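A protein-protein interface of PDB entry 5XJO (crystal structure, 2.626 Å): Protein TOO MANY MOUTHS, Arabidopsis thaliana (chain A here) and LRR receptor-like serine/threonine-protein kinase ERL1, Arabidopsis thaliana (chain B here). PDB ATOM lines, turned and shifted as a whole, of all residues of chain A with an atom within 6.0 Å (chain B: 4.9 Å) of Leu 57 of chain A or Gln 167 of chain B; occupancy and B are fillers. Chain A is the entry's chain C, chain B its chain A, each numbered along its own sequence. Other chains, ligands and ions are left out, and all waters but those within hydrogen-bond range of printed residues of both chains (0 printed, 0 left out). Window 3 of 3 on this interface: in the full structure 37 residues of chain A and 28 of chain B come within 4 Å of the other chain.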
ATOM      1  N   GLY A  55     -11.311  16.506  -2.409  1.00  0.00           N
ATOM      2  CA  GLY A  55     -10.445  17.512  -1.877  1.00  0.00           C
ATOM      3  C   GLY A  55     -10.784  18.903  -2.275  1.00  0.00           C
ATOM      4  O   GLY A  55     -11.417  19.136  -3.269  1.00  0.00           O
ATOM      5  N   ALA A  56     -10.343  19.838  -1.480  1.00  0.00           N
ATOM      6  CA  ALA A  56     -10.647  21.185  -1.787  1.00  0.00           C
ATOM      7  C   ALA A  56      -9.467  21.759  -2.455  1.00  0.00           C
ATOM      8  O   ALA A  56      -8.529  22.128  -1.787  1.00  0.00           O
ATOM      9  CB  ALA A  56     -10.917  21.944  -0.517  1.00  0.00           C
ATOM     10  N   LEU A  57      -9.547  21.943  -3.772  1.00  0.00           N
ATOM     11  CA  LEU A  57      -8.483  22.525  -4.580  1.00  0.00           C
ATOM     12  C   LEU A  57      -8.657  24.037  -4.578  1.00  0.00           C
ATOM     13  O   LEU A  57      -8.857  24.592  -5.619  1.00  0.00           O
ATOM     14  CB  LEU A  57      -8.575  21.964  -6.011  1.00  0.00           C
ATOM     15  CG  LEU A  57      -7.644  22.278  -7.209  1.00  0.00           C
ATOM     16  CD1 LEU A  57      -6.289  21.652  -7.010  1.00  0.00           C
ATOM     17  CD2 LEU A  57      -8.160  21.911  -8.608  1.00  0.00           C
ATOM     18  N   SER A  58      -8.461  24.649  -3.404  1.00  0.00           N
ATOM     19  CA  SER A  58      -8.662  26.032  -2.970  1.00  0.00           C
ATOM     20  C   SER A  58     -10.060  26.437  -2.514  1.00  0.00           C
ATOM     21  O   SER A  58     -10.347  27.610  -2.484  1.00  0.00           O
ATOM     22  CB  SER A  58      -7.996  27.101  -3.840  1.00  0.00           C
ATOM     23  N   ASP A  59     -10.976  25.496  -2.356  1.00  0.00           N
ATOM     24  CA  ASP A  59     -12.311  25.733  -1.755  1.00  0.00           C
ATOM     25  C   ASP A  59     -13.370  26.630  -2.479  1.00  0.00           C
ATOM     26  O   ASP A  59     -14.494  26.797  -2.013  1.00  0.00           O
ATOM     27  CB  ASP A  59     -12.191  26.087  -0.267  1.00  0.00           C
ATOM     28  CG  ASP A  59     -13.344  25.505   0.592  1.00  0.00           C
ATOM     29  OD1 ASP A  59     -14.527  25.758   0.295  1.00  0.00           O
ATOM     30  OD2 ASP A  59     -13.072  24.806   1.585  1.00  0.00           O
ATOM     31  N   ASP A  60     -13.004  27.221  -3.611  1.00  0.00           N
ATOM     32  CA  ASP A  60     -13.954  28.008  -4.341  1.00  0.00           C
ATOM     33  C   ASP A  60     -14.904  26.983  -4.878  1.00  0.00           C
ATOM     34  O   ASP A  60     -16.066  27.013  -4.603  1.00  0.00           O
ATOM     35  CB  ASP A  60     -13.230  28.655  -5.520  1.00  0.00           C
ATOM     36  CG  ASP A  60     -12.272  29.749  -5.127  1.00  0.00           C
ATOM     37  OD1 ASP A  60     -12.348  30.219  -3.997  1.00  0.00           O
ATOM     38  OD2 ASP A  60     -11.485  30.195  -5.970  1.00  0.00           O
ATOM     39  N   THR A  61     -14.337  25.966  -5.503  1.00  0.00           N
ATOM     40  CA  THR A  61     -15.079  24.905  -6.133  1.00  0.00           C
ATOM     41  C   THR A  61     -14.477  23.625  -5.600  1.00  0.00           C
ATOM     42  O   THR A  61     -13.811  22.887  -6.281  1.00  0.00           O
ATOM     43  CB  THR A  61     -14.997  24.997  -7.677  1.00  0.00           C
ATOM     44  OG1 THR A  61     -14.907  26.364  -8.070  1.00  0.00           O
ATOM     45  CG2 THR A  61     -16.242  24.473  -8.315  1.00  0.00           C
ATOM     46  N   ALA A  62     -14.732  23.423  -4.320  1.00  0.00           N
ATOM     47  CA  ALA A  62     -14.301  22.273  -3.550  1.00  0.00           C
ATOM     48  C   ALA A  62     -15.008  20.953  -3.745  1.00  0.00           C
ATOM     49  O   ALA A  62     -16.194  20.857  -3.958  1.00  0.00           O
ATOM     50  CB  ALA A  62     -14.289  22.611  -2.074  1.00  0.00           C
ATOM     51  N   PHE A  63     -14.218  19.921  -3.595  1.00  0.00           N
ATOM     52  CA  PHE A  63     -14.689  18.584  -3.691  1.00  0.00           C
ATOM     53  C   PHE A  63     -14.923  18.048  -2.304  1.00  0.00           C
ATOM     54  O   PHE A  63     -14.553  18.626  -1.342  1.00  0.00           O
ATOM     55  CB  PHE A  63     -13.697  17.701  -4.416  1.00  0.00           C
ATOM     56  CG  PHE A  63     -13.488  18.056  -5.835  1.00  0.00           C
ATOM     57  CD1 PHE A  63     -14.541  18.212  -6.674  1.00  0.00           C
ATOM     58  CD2 PHE A  63     -12.226  18.199  -6.323  1.00  0.00           C
ATOM     59  CE1 PHE A  63     -14.351  18.522  -7.986  1.00  0.00           C
ATOM     60  CE2 PHE A  63     -12.014  18.522  -7.627  1.00  0.00           C
ATOM     61  CZ  PHE A  63     -13.083  18.688  -8.464  1.00  0.00           C
ATOM     62  N   PHE A  87      -9.194  11.750  -8.834  1.00  0.00           N
ATOM     63  CA  PHE A  87      -8.530  12.955  -8.367  1.00  0.00           C
ATOM     64  C   PHE A  87      -8.630  12.955  -6.848  1.00  0.00           C
ATOM     65  O   PHE A  87      -9.716  12.731  -6.296  1.00  0.00           O
ATOM     66  CB  PHE A  87      -9.200  14.176  -9.035  1.00  0.00           C
ATOM     67  CG  PHE A  87      -8.627  15.534  -8.680  1.00  0.00           C
ATOM     68  CD1 PHE A  87      -8.836  16.111  -7.440  1.00  0.00           C
ATOM     69  CD2 PHE A  87      -7.942  16.272  -9.632  1.00  0.00           C
ATOM     70  CE1 PHE A  87      -8.331  17.398  -7.154  1.00  0.00           C
ATOM     71  CE2 PHE A  87      -7.416  17.547  -9.334  1.00  0.00           C
ATOM     72  CZ  PHE A  87      -7.611  18.097  -8.100  1.00  0.00           C
ATOM     73  N   TYR A  89      -6.929  15.346  -3.685  1.00  0.00           N
ATOM     74  CA  TYR A  89      -6.080  16.507  -3.459  1.00  0.00           C
ATOM     75  C   TYR A  89      -6.155  16.943  -2.007  1.00  0.00           C
ATOM     76  O   TYR A  89      -7.212  17.371  -1.539  1.00  0.00           O
ATOM     77  CB  TYR A  89      -6.497  17.632  -4.383  1.00  0.00           C
ATOM     78  CG  TYR A  89      -5.705  18.880  -4.205  1.00  0.00           C
ATOM     79  CD1 TYR A  89      -6.208  19.936  -3.462  1.00  0.00           C
ATOM     80  CD2 TYR A  89      -4.454  19.008  -4.788  1.00  0.00           C
ATOM     81  CE1 TYR A  89      -5.497  21.070  -3.308  1.00  0.00           C
ATOM     82  CE2 TYR A  89      -3.738  20.140  -4.641  1.00  0.00           C
ATOM     83  CZ  TYR A  89      -4.263  21.164  -3.902  1.00  0.00           C
ATOM     84  OH  TYR A  89      -3.554  22.307  -3.760  1.00  0.00           O
ATOM     85  N   ARG A 116      -2.542  13.926  -5.374  1.00  0.00           N
ATOM     86  CA  ARG A 116      -1.676  15.071  -5.173  1.00  0.00           C
ATOM     87  C   ARG A 116      -1.711  15.482  -3.712  1.00  0.00           C
ATOM     88  O   ARG A 116      -2.767  15.836  -3.189  1.00  0.00           O
ATOM     89  CB  ARG A 116      -2.126  16.210  -6.084  1.00  0.00           C
ATOM     90  CG  ARG A 116      -1.057  17.220  -6.453  1.00  0.00           C
ATOM     91  CD  ARG A 116      -1.602  18.294  -7.410  1.00  0.00           C
ATOM     92  NE  ARG A 116      -0.822  19.524  -7.321  1.00  0.00           N
ATOM     93  CZ  ARG A 116       0.127  19.857  -8.186  1.00  0.00           C
ATOM     94  NH1 ARG A 116       0.400  19.063  -9.195  1.00  0.00           N
ATOM     95  NH2 ARG A 116       0.805  20.978  -8.042  1.00  0.00           N
ATOM     96  N   LYS B 143      -2.795  29.291  -7.724  1.00  0.00           N
ATOM     97  CA  LYS B 143      -4.213  29.104  -7.991  1.00  0.00           C
ATOM     98  C   LYS B 143      -4.884  30.283  -8.678  1.00  0.00           C
ATOM     99  O   LYS B 143      -5.811  30.077  -9.469  1.00  0.00           O
ATOM    100  CB  LYS B 143      -4.944  28.796  -6.689  1.00  0.00           C
ATOM    101  CG  LYS B 143      -4.634  27.433  -6.170  1.00  0.00           C
ATOM    102  CD  LYS B 143      -5.112  27.246  -4.778  1.00  0.00           C
ATOM    103  CE  LYS B 143      -4.359  26.091  -4.146  1.00  0.00           C
ATOM    104  NZ  LYS B 143      -4.656  24.816  -4.857  1.00  0.00           N
ATOM    105  N   GLU B 164      -3.049  21.580 -13.608  1.00  0.00           N
ATOM    106  CA  GLU B 164      -4.266  21.021 -13.051  1.00  0.00           C
ATOM    107  C   GLU B 164      -4.807  21.837 -11.883  1.00  0.00           C
ATOM    108  O   GLU B 164      -5.990  21.673 -11.529  1.00  0.00           O
ATOM    109  CB  GLU B 164      -4.007  19.550 -12.629  1.00  0.00           C
ATOM    110  CG  GLU B 164      -5.201  18.742 -12.002  1.00  0.00           C
ATOM    111  CD  GLU B 164      -6.626  19.193 -12.468  1.00  0.00           C
ATOM    112  OE1 GLU B 164      -6.815  19.483 -13.664  1.00  0.00           O
ATOM    113  OE2 GLU B 164      -7.556  19.216 -11.637  1.00  0.00           O
ATOM    114  N   VAL B 165      -3.992  22.736 -11.325  1.00  0.00           N
ATOM    115  CA  VAL B 165      -4.306  23.420 -10.074  1.00  0.00           C
ATOM    116  C   VAL B 165      -4.868  24.816 -10.298  1.00  0.00           C
ATOM    117  O   VAL B 165      -5.648  25.313  -9.478  1.00  0.00           O
ATOM    118  CB  VAL B 165      -3.046  23.531  -9.186  1.00  0.00           C
ATOM    119  CG1 VAL B 165      -3.399  23.976  -7.742  1.00  0.00           C
ATOM    120  CG2 VAL B 165      -2.265  22.233  -9.186  1.00  0.00           C
ATOM    121  N   LEU B 166      -4.481  25.456 -11.405  1.00  0.00           N
ATOM    122  CA  LEU B 166      -4.856  26.846 -11.654  1.00  0.00           C
ATOM    123  C   LEU B 166      -6.364  27.018 -11.750  1.00  0.00           C
ATOM    124  O   LEU B 166      -7.025  26.319 -12.518  1.00  0.00           O
ATOM    125  CB  LEU B 166      -4.204  27.347 -12.935  1.00  0.00           C
ATOM    126  CG  LEU B 166      -4.202  28.869 -13.024  1.00  0.00           C
ATOM    127  CD1 LEU B 166      -3.213  29.425 -12.017  1.00  0.00           C
ATOM    128  CD2 LEU B 166      -3.881  29.250 -14.419  1.00  0.00           C
ATOM    129  N   GLN B 167      -6.884  27.995 -10.997  1.00  0.00           N
ATOM    130  CA  GLN B 167      -8.308  28.293 -10.864  1.00  0.00           C
ATOM    131  C   GLN B 167      -8.716  29.490 -11.713  1.00  0.00           C
ATOM    132  O   GLN B 167      -9.658  29.419 -12.509  1.00  0.00           O
ATOM    133  CB  GLN B 167      -8.637  28.608  -9.402  1.00  0.00           C
ATOM    134  CG  GLN B 167      -8.113  27.616  -8.391  1.00  0.00           C
ATOM    135  CD  GLN B 167      -9.107  26.519  -8.147  1.00  0.00           C
ATOM    136  OE1 GLN B 167      -8.969  25.407  -8.677  1.00  0.00           O
ATOM    137  NE2 GLN B 167     -10.149  26.829  -7.365  1.00  0.00           N
ATOM    138  N   TYR B 168      -8.031  30.609 -11.510  1.00  0.00           N
ATOM    139  CA  TYR B 168      -8.338  31.882 -12.124  1.00  0.00           C
ATOM    140  C   TYR B 168      -7.161  32.275 -13.004  1.00  0.00           C
ATOM    141  O   TYR B 168      -6.018  32.342 -12.525  1.00  0.00           O
ATOM    142  CB  TYR B 168      -8.588  32.928 -11.041  1.00  0.00           C
ATOM    143  CG  TYR B 168      -8.907  34.362 -11.476  1.00  0.00           C
ATOM    144  CD1 TYR B 168      -7.940  35.178 -12.048  1.00  0.00           C
ATOM    145  CD2 TYR B 168     -10.158  34.923 -11.202  1.00  0.00           C
ATOM    146  CE1 TYR B 168      -8.234  36.511 -12.399  1.00  0.00           C
ATOM    147  CE2 TYR B 168     -10.456  36.248 -11.537  1.00  0.00           C
ATOM    148  CZ  TYR B 168      -9.498  37.036 -12.137  1.00  0.00           C
ATOM    149  OH  TYR B 168      -9.798  38.332 -12.470  1.00  0.00           O
ATOM    150  N   LEU B 169      -7.451  32.536 -14.279  1.00  0.00           N
ATOM    151  CA  LEU B 169      -6.459  32.993 -15.248  1.00  0.00           C
ATOM    152  C   LEU B 169      -6.981  34.309 -15.802  1.00  0.00           C
ATOM    153  O   LEU B 169      -7.871  34.309 -16.657  1.00  0.00           O
ATOM    154  CB  LEU B 169      -6.246  31.993 -16.367  1.00  0.00           C
ATOM    155  CG  LEU B 169      -5.233  32.542 -17.363  1.00  0.00           C
ATOM    156  CD1 LEU B 169      -3.863  32.650 -16.663  1.00  0.00           C
ATOM    157  CD2 LEU B 169      -5.141  31.705 -18.650  1.00  0.00           C
ATOM    158  N   GLY B 189      -8.792  22.480 -13.856  1.00  0.00           N
ATOM    159  CA  GLY B 189      -9.419  22.861 -12.604  1.00  0.00           C
ATOM    160  C   GLY B 189      -9.777  24.333 -12.547  1.00  0.00           C
ATOM    161  O   GLY B 189     -10.125  24.875 -11.487  1.00  0.00           O
ATOM    162  N   LEU B 190      -9.743  24.958 -13.725  1.00  0.00           N
ATOM    163  CA  LEU B 190      -9.905  26.391 -13.902  1.00  0.00           C
ATOM    164  C   LEU B 190     -11.366  26.720 -14.180  1.00  0.00           C
ATOM    165  O   LEU B 190     -12.018  26.070 -15.003  1.00  0.00           O
ATOM    166  CB  LEU B 190      -8.991  26.864 -15.036  1.00  0.00           C
ATOM    167  CG  LEU B 190      -8.919  28.359 -15.343  1.00  0.00           C
ATOM    168  CD1 LEU B 190      -7.514  28.858 -15.168  1.00  0.00           C
ATOM    169  CD2 LEU B 190      -9.324  28.629 -16.778  1.00  0.00           C
ATOM    170  N   TRP B 191     -11.888  27.720 -13.478  1.00  0.00           N
ATOM    171  CA  TRP B 191     -13.232  28.180 -13.753  1.00  0.00           C
ATOM    172  C   TRP B 191     -13.281  29.531 -14.451  1.00  0.00           C
ATOM    173  O   TRP B 191     -14.341  29.905 -14.965  1.00  0.00           O
ATOM    174  CB  TRP B 191     -14.048  28.247 -12.456  1.00  0.00           C
ATOM    175  CG  TRP B 191     -13.524  29.165 -11.423  1.00  0.00           C
ATOM    176  CD1 TRP B 191     -12.582  28.887 -10.489  1.00  0.00           C
ATOM    177  CD2 TRP B 191     -13.914  30.519 -11.207  1.00  0.00           C
ATOM    178  NE1 TRP B 191     -12.366  29.983  -9.690  1.00  0.00           N
ATOM    179  CE2 TRP B 191     -13.168  31.003 -10.119  1.00  0.00           C
ATOM    180  CE3 TRP B 191     -14.829  31.366 -11.818  1.00  0.00           C
ATOM    181  CZ2 TRP B 191     -13.297  32.294  -9.638  1.00  0.00           C
ATOM    182  CZ3 TRP B 191     -14.965  32.664 -11.327  1.00  0.00           C
ATOM    183  CH2 TRP B 191     -14.205  33.106 -10.246  1.00  0.00           C
ATOM    184  N   TYR B 192     -12.175  30.265 -14.508  1.00  0.00           N
ATOM    185  CA  TYR B 192     -12.179  31.632 -15.024  1.00  0.00           C
ATOM    186  C   TYR B 192     -11.053  31.752 -16.034  1.00  0.00           C
ATOM    187  O   TYR B 192      -9.876  31.692 -15.655  1.00  0.00           O
ATOM    188  CB  TYR B 192     -12.010  32.653 -13.891  1.00  0.00           C
ATOM    189  CG  TYR B 192     -12.122  34.118 -14.314  1.00  0.00           C
ATOM    190  CD1 TYR B 192     -13.366  34.775 -14.374  1.00  0.00           C
ATOM    191  CD2 TYR B 192     -10.988  34.849 -14.636  1.00  0.00           C
ATOM    192  CE1 TYR B 192     -13.452  36.095 -14.743  1.00  0.00           C
ATOM    193  CE2 TYR B 192     -11.072  36.168 -14.997  1.00  0.00           C
ATOM    194  CZ  TYR B 192     -12.300  36.780 -15.070  1.00  0.00           C
ATOM    195  OH  TYR B 192     -12.344  38.096 -15.454  1.00  0.00           O
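The side-chain amide nitrogen (NE2) of Gln 167 of chain B sits at hydrogen-bond distance from the backbone carbonyl oxygen (O) of Leu 57 of chain A (3.1 Å).
The side-chain amino group of Lys 143 of chain B is in hydrogen-bond range of the side-chain hydroxyl of Tyr 89 of chain A.
Hydrophobic or aromatic side chains of chain A within 4 Å of the printed part of chain B: Leu 57, Phe 87 and Tyr 89.
Along chain A the printed residues that touch a printed residue of chain B span positions 57 to 116.
Of the 11 printed residues of chain B, 5 touch a printed residue of chain A.
Hydrophobic or aromatic side chains of chain B that line the printed part of chain A: Val 165 and Trp 191.
Among the printed residues, no Asp or Glu carboxylate lies within 4 Å of a Lys or Arg side-chain nitrogen of the other chain.
Among the printed residues, pairs that only touch across the chains: Phe 87 of chain A with Glu 164 of chain B, Ser 58 of chain A with Lys 143 of chain B, Arg 116 of chain A with Val 165 of chain B, Leu 57 of chain A with Glu 164 of chain B, Leu 57 of chain A with Val 165 of chain B, Asp 60 of chain A with Trp 191 of chain B and Asp 60 of chain A with Gln 167 of chain B.
Gly 55 of chain A touches none of the printed residues of chain B.
Leu 57 of chain A touches just these residues of chain B: Glu 164, Val 165 and Gln 167.
Of the printed residues of chain B, Asp 60 of chain A touches Gln 167 and Trp 191.
Of the printed residues of chain B, Tyr 89 of chain A touches Lys 143 (3.0 Å).
Gln 167 of chain B touches two residues of chain A.
The backbone carbonyl oxygen (O) of Lys 143 of chain B lies within hydrogen-bond range of the backbone NH (N) of Tyr 168 of chain B (3.1 Å).
The side-chain amide oxygen (OE1) of Gln 167 of chain B sits close to the backbone carbonyl oxygen (O) of Gly 189 of chain B (3.1 Å).
The side-chain amide oxygen (OE1) of Gln 167 of chain B lies close to the backbone carbonyl oxygen (O) of Val 165 of chain B.
The backbone NH (N) of Tyr 192 of chain B sits at hydrogen-bond distance from the backbone carbonyl oxygen (O) of Gln 167 of chain B (3.3 Å).
The backbone NH (N) of Trp 191 of chain B lies within hydrogen-bond range of the backbone carbonyl oxygen (O) of Gln 167 of chain B, 3.0 Å away.
The backbone NH of Gln 167 of chain B sits at hydrogen-bond distance from the backbone carbonyl oxygen of Lys 143 of chain B.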
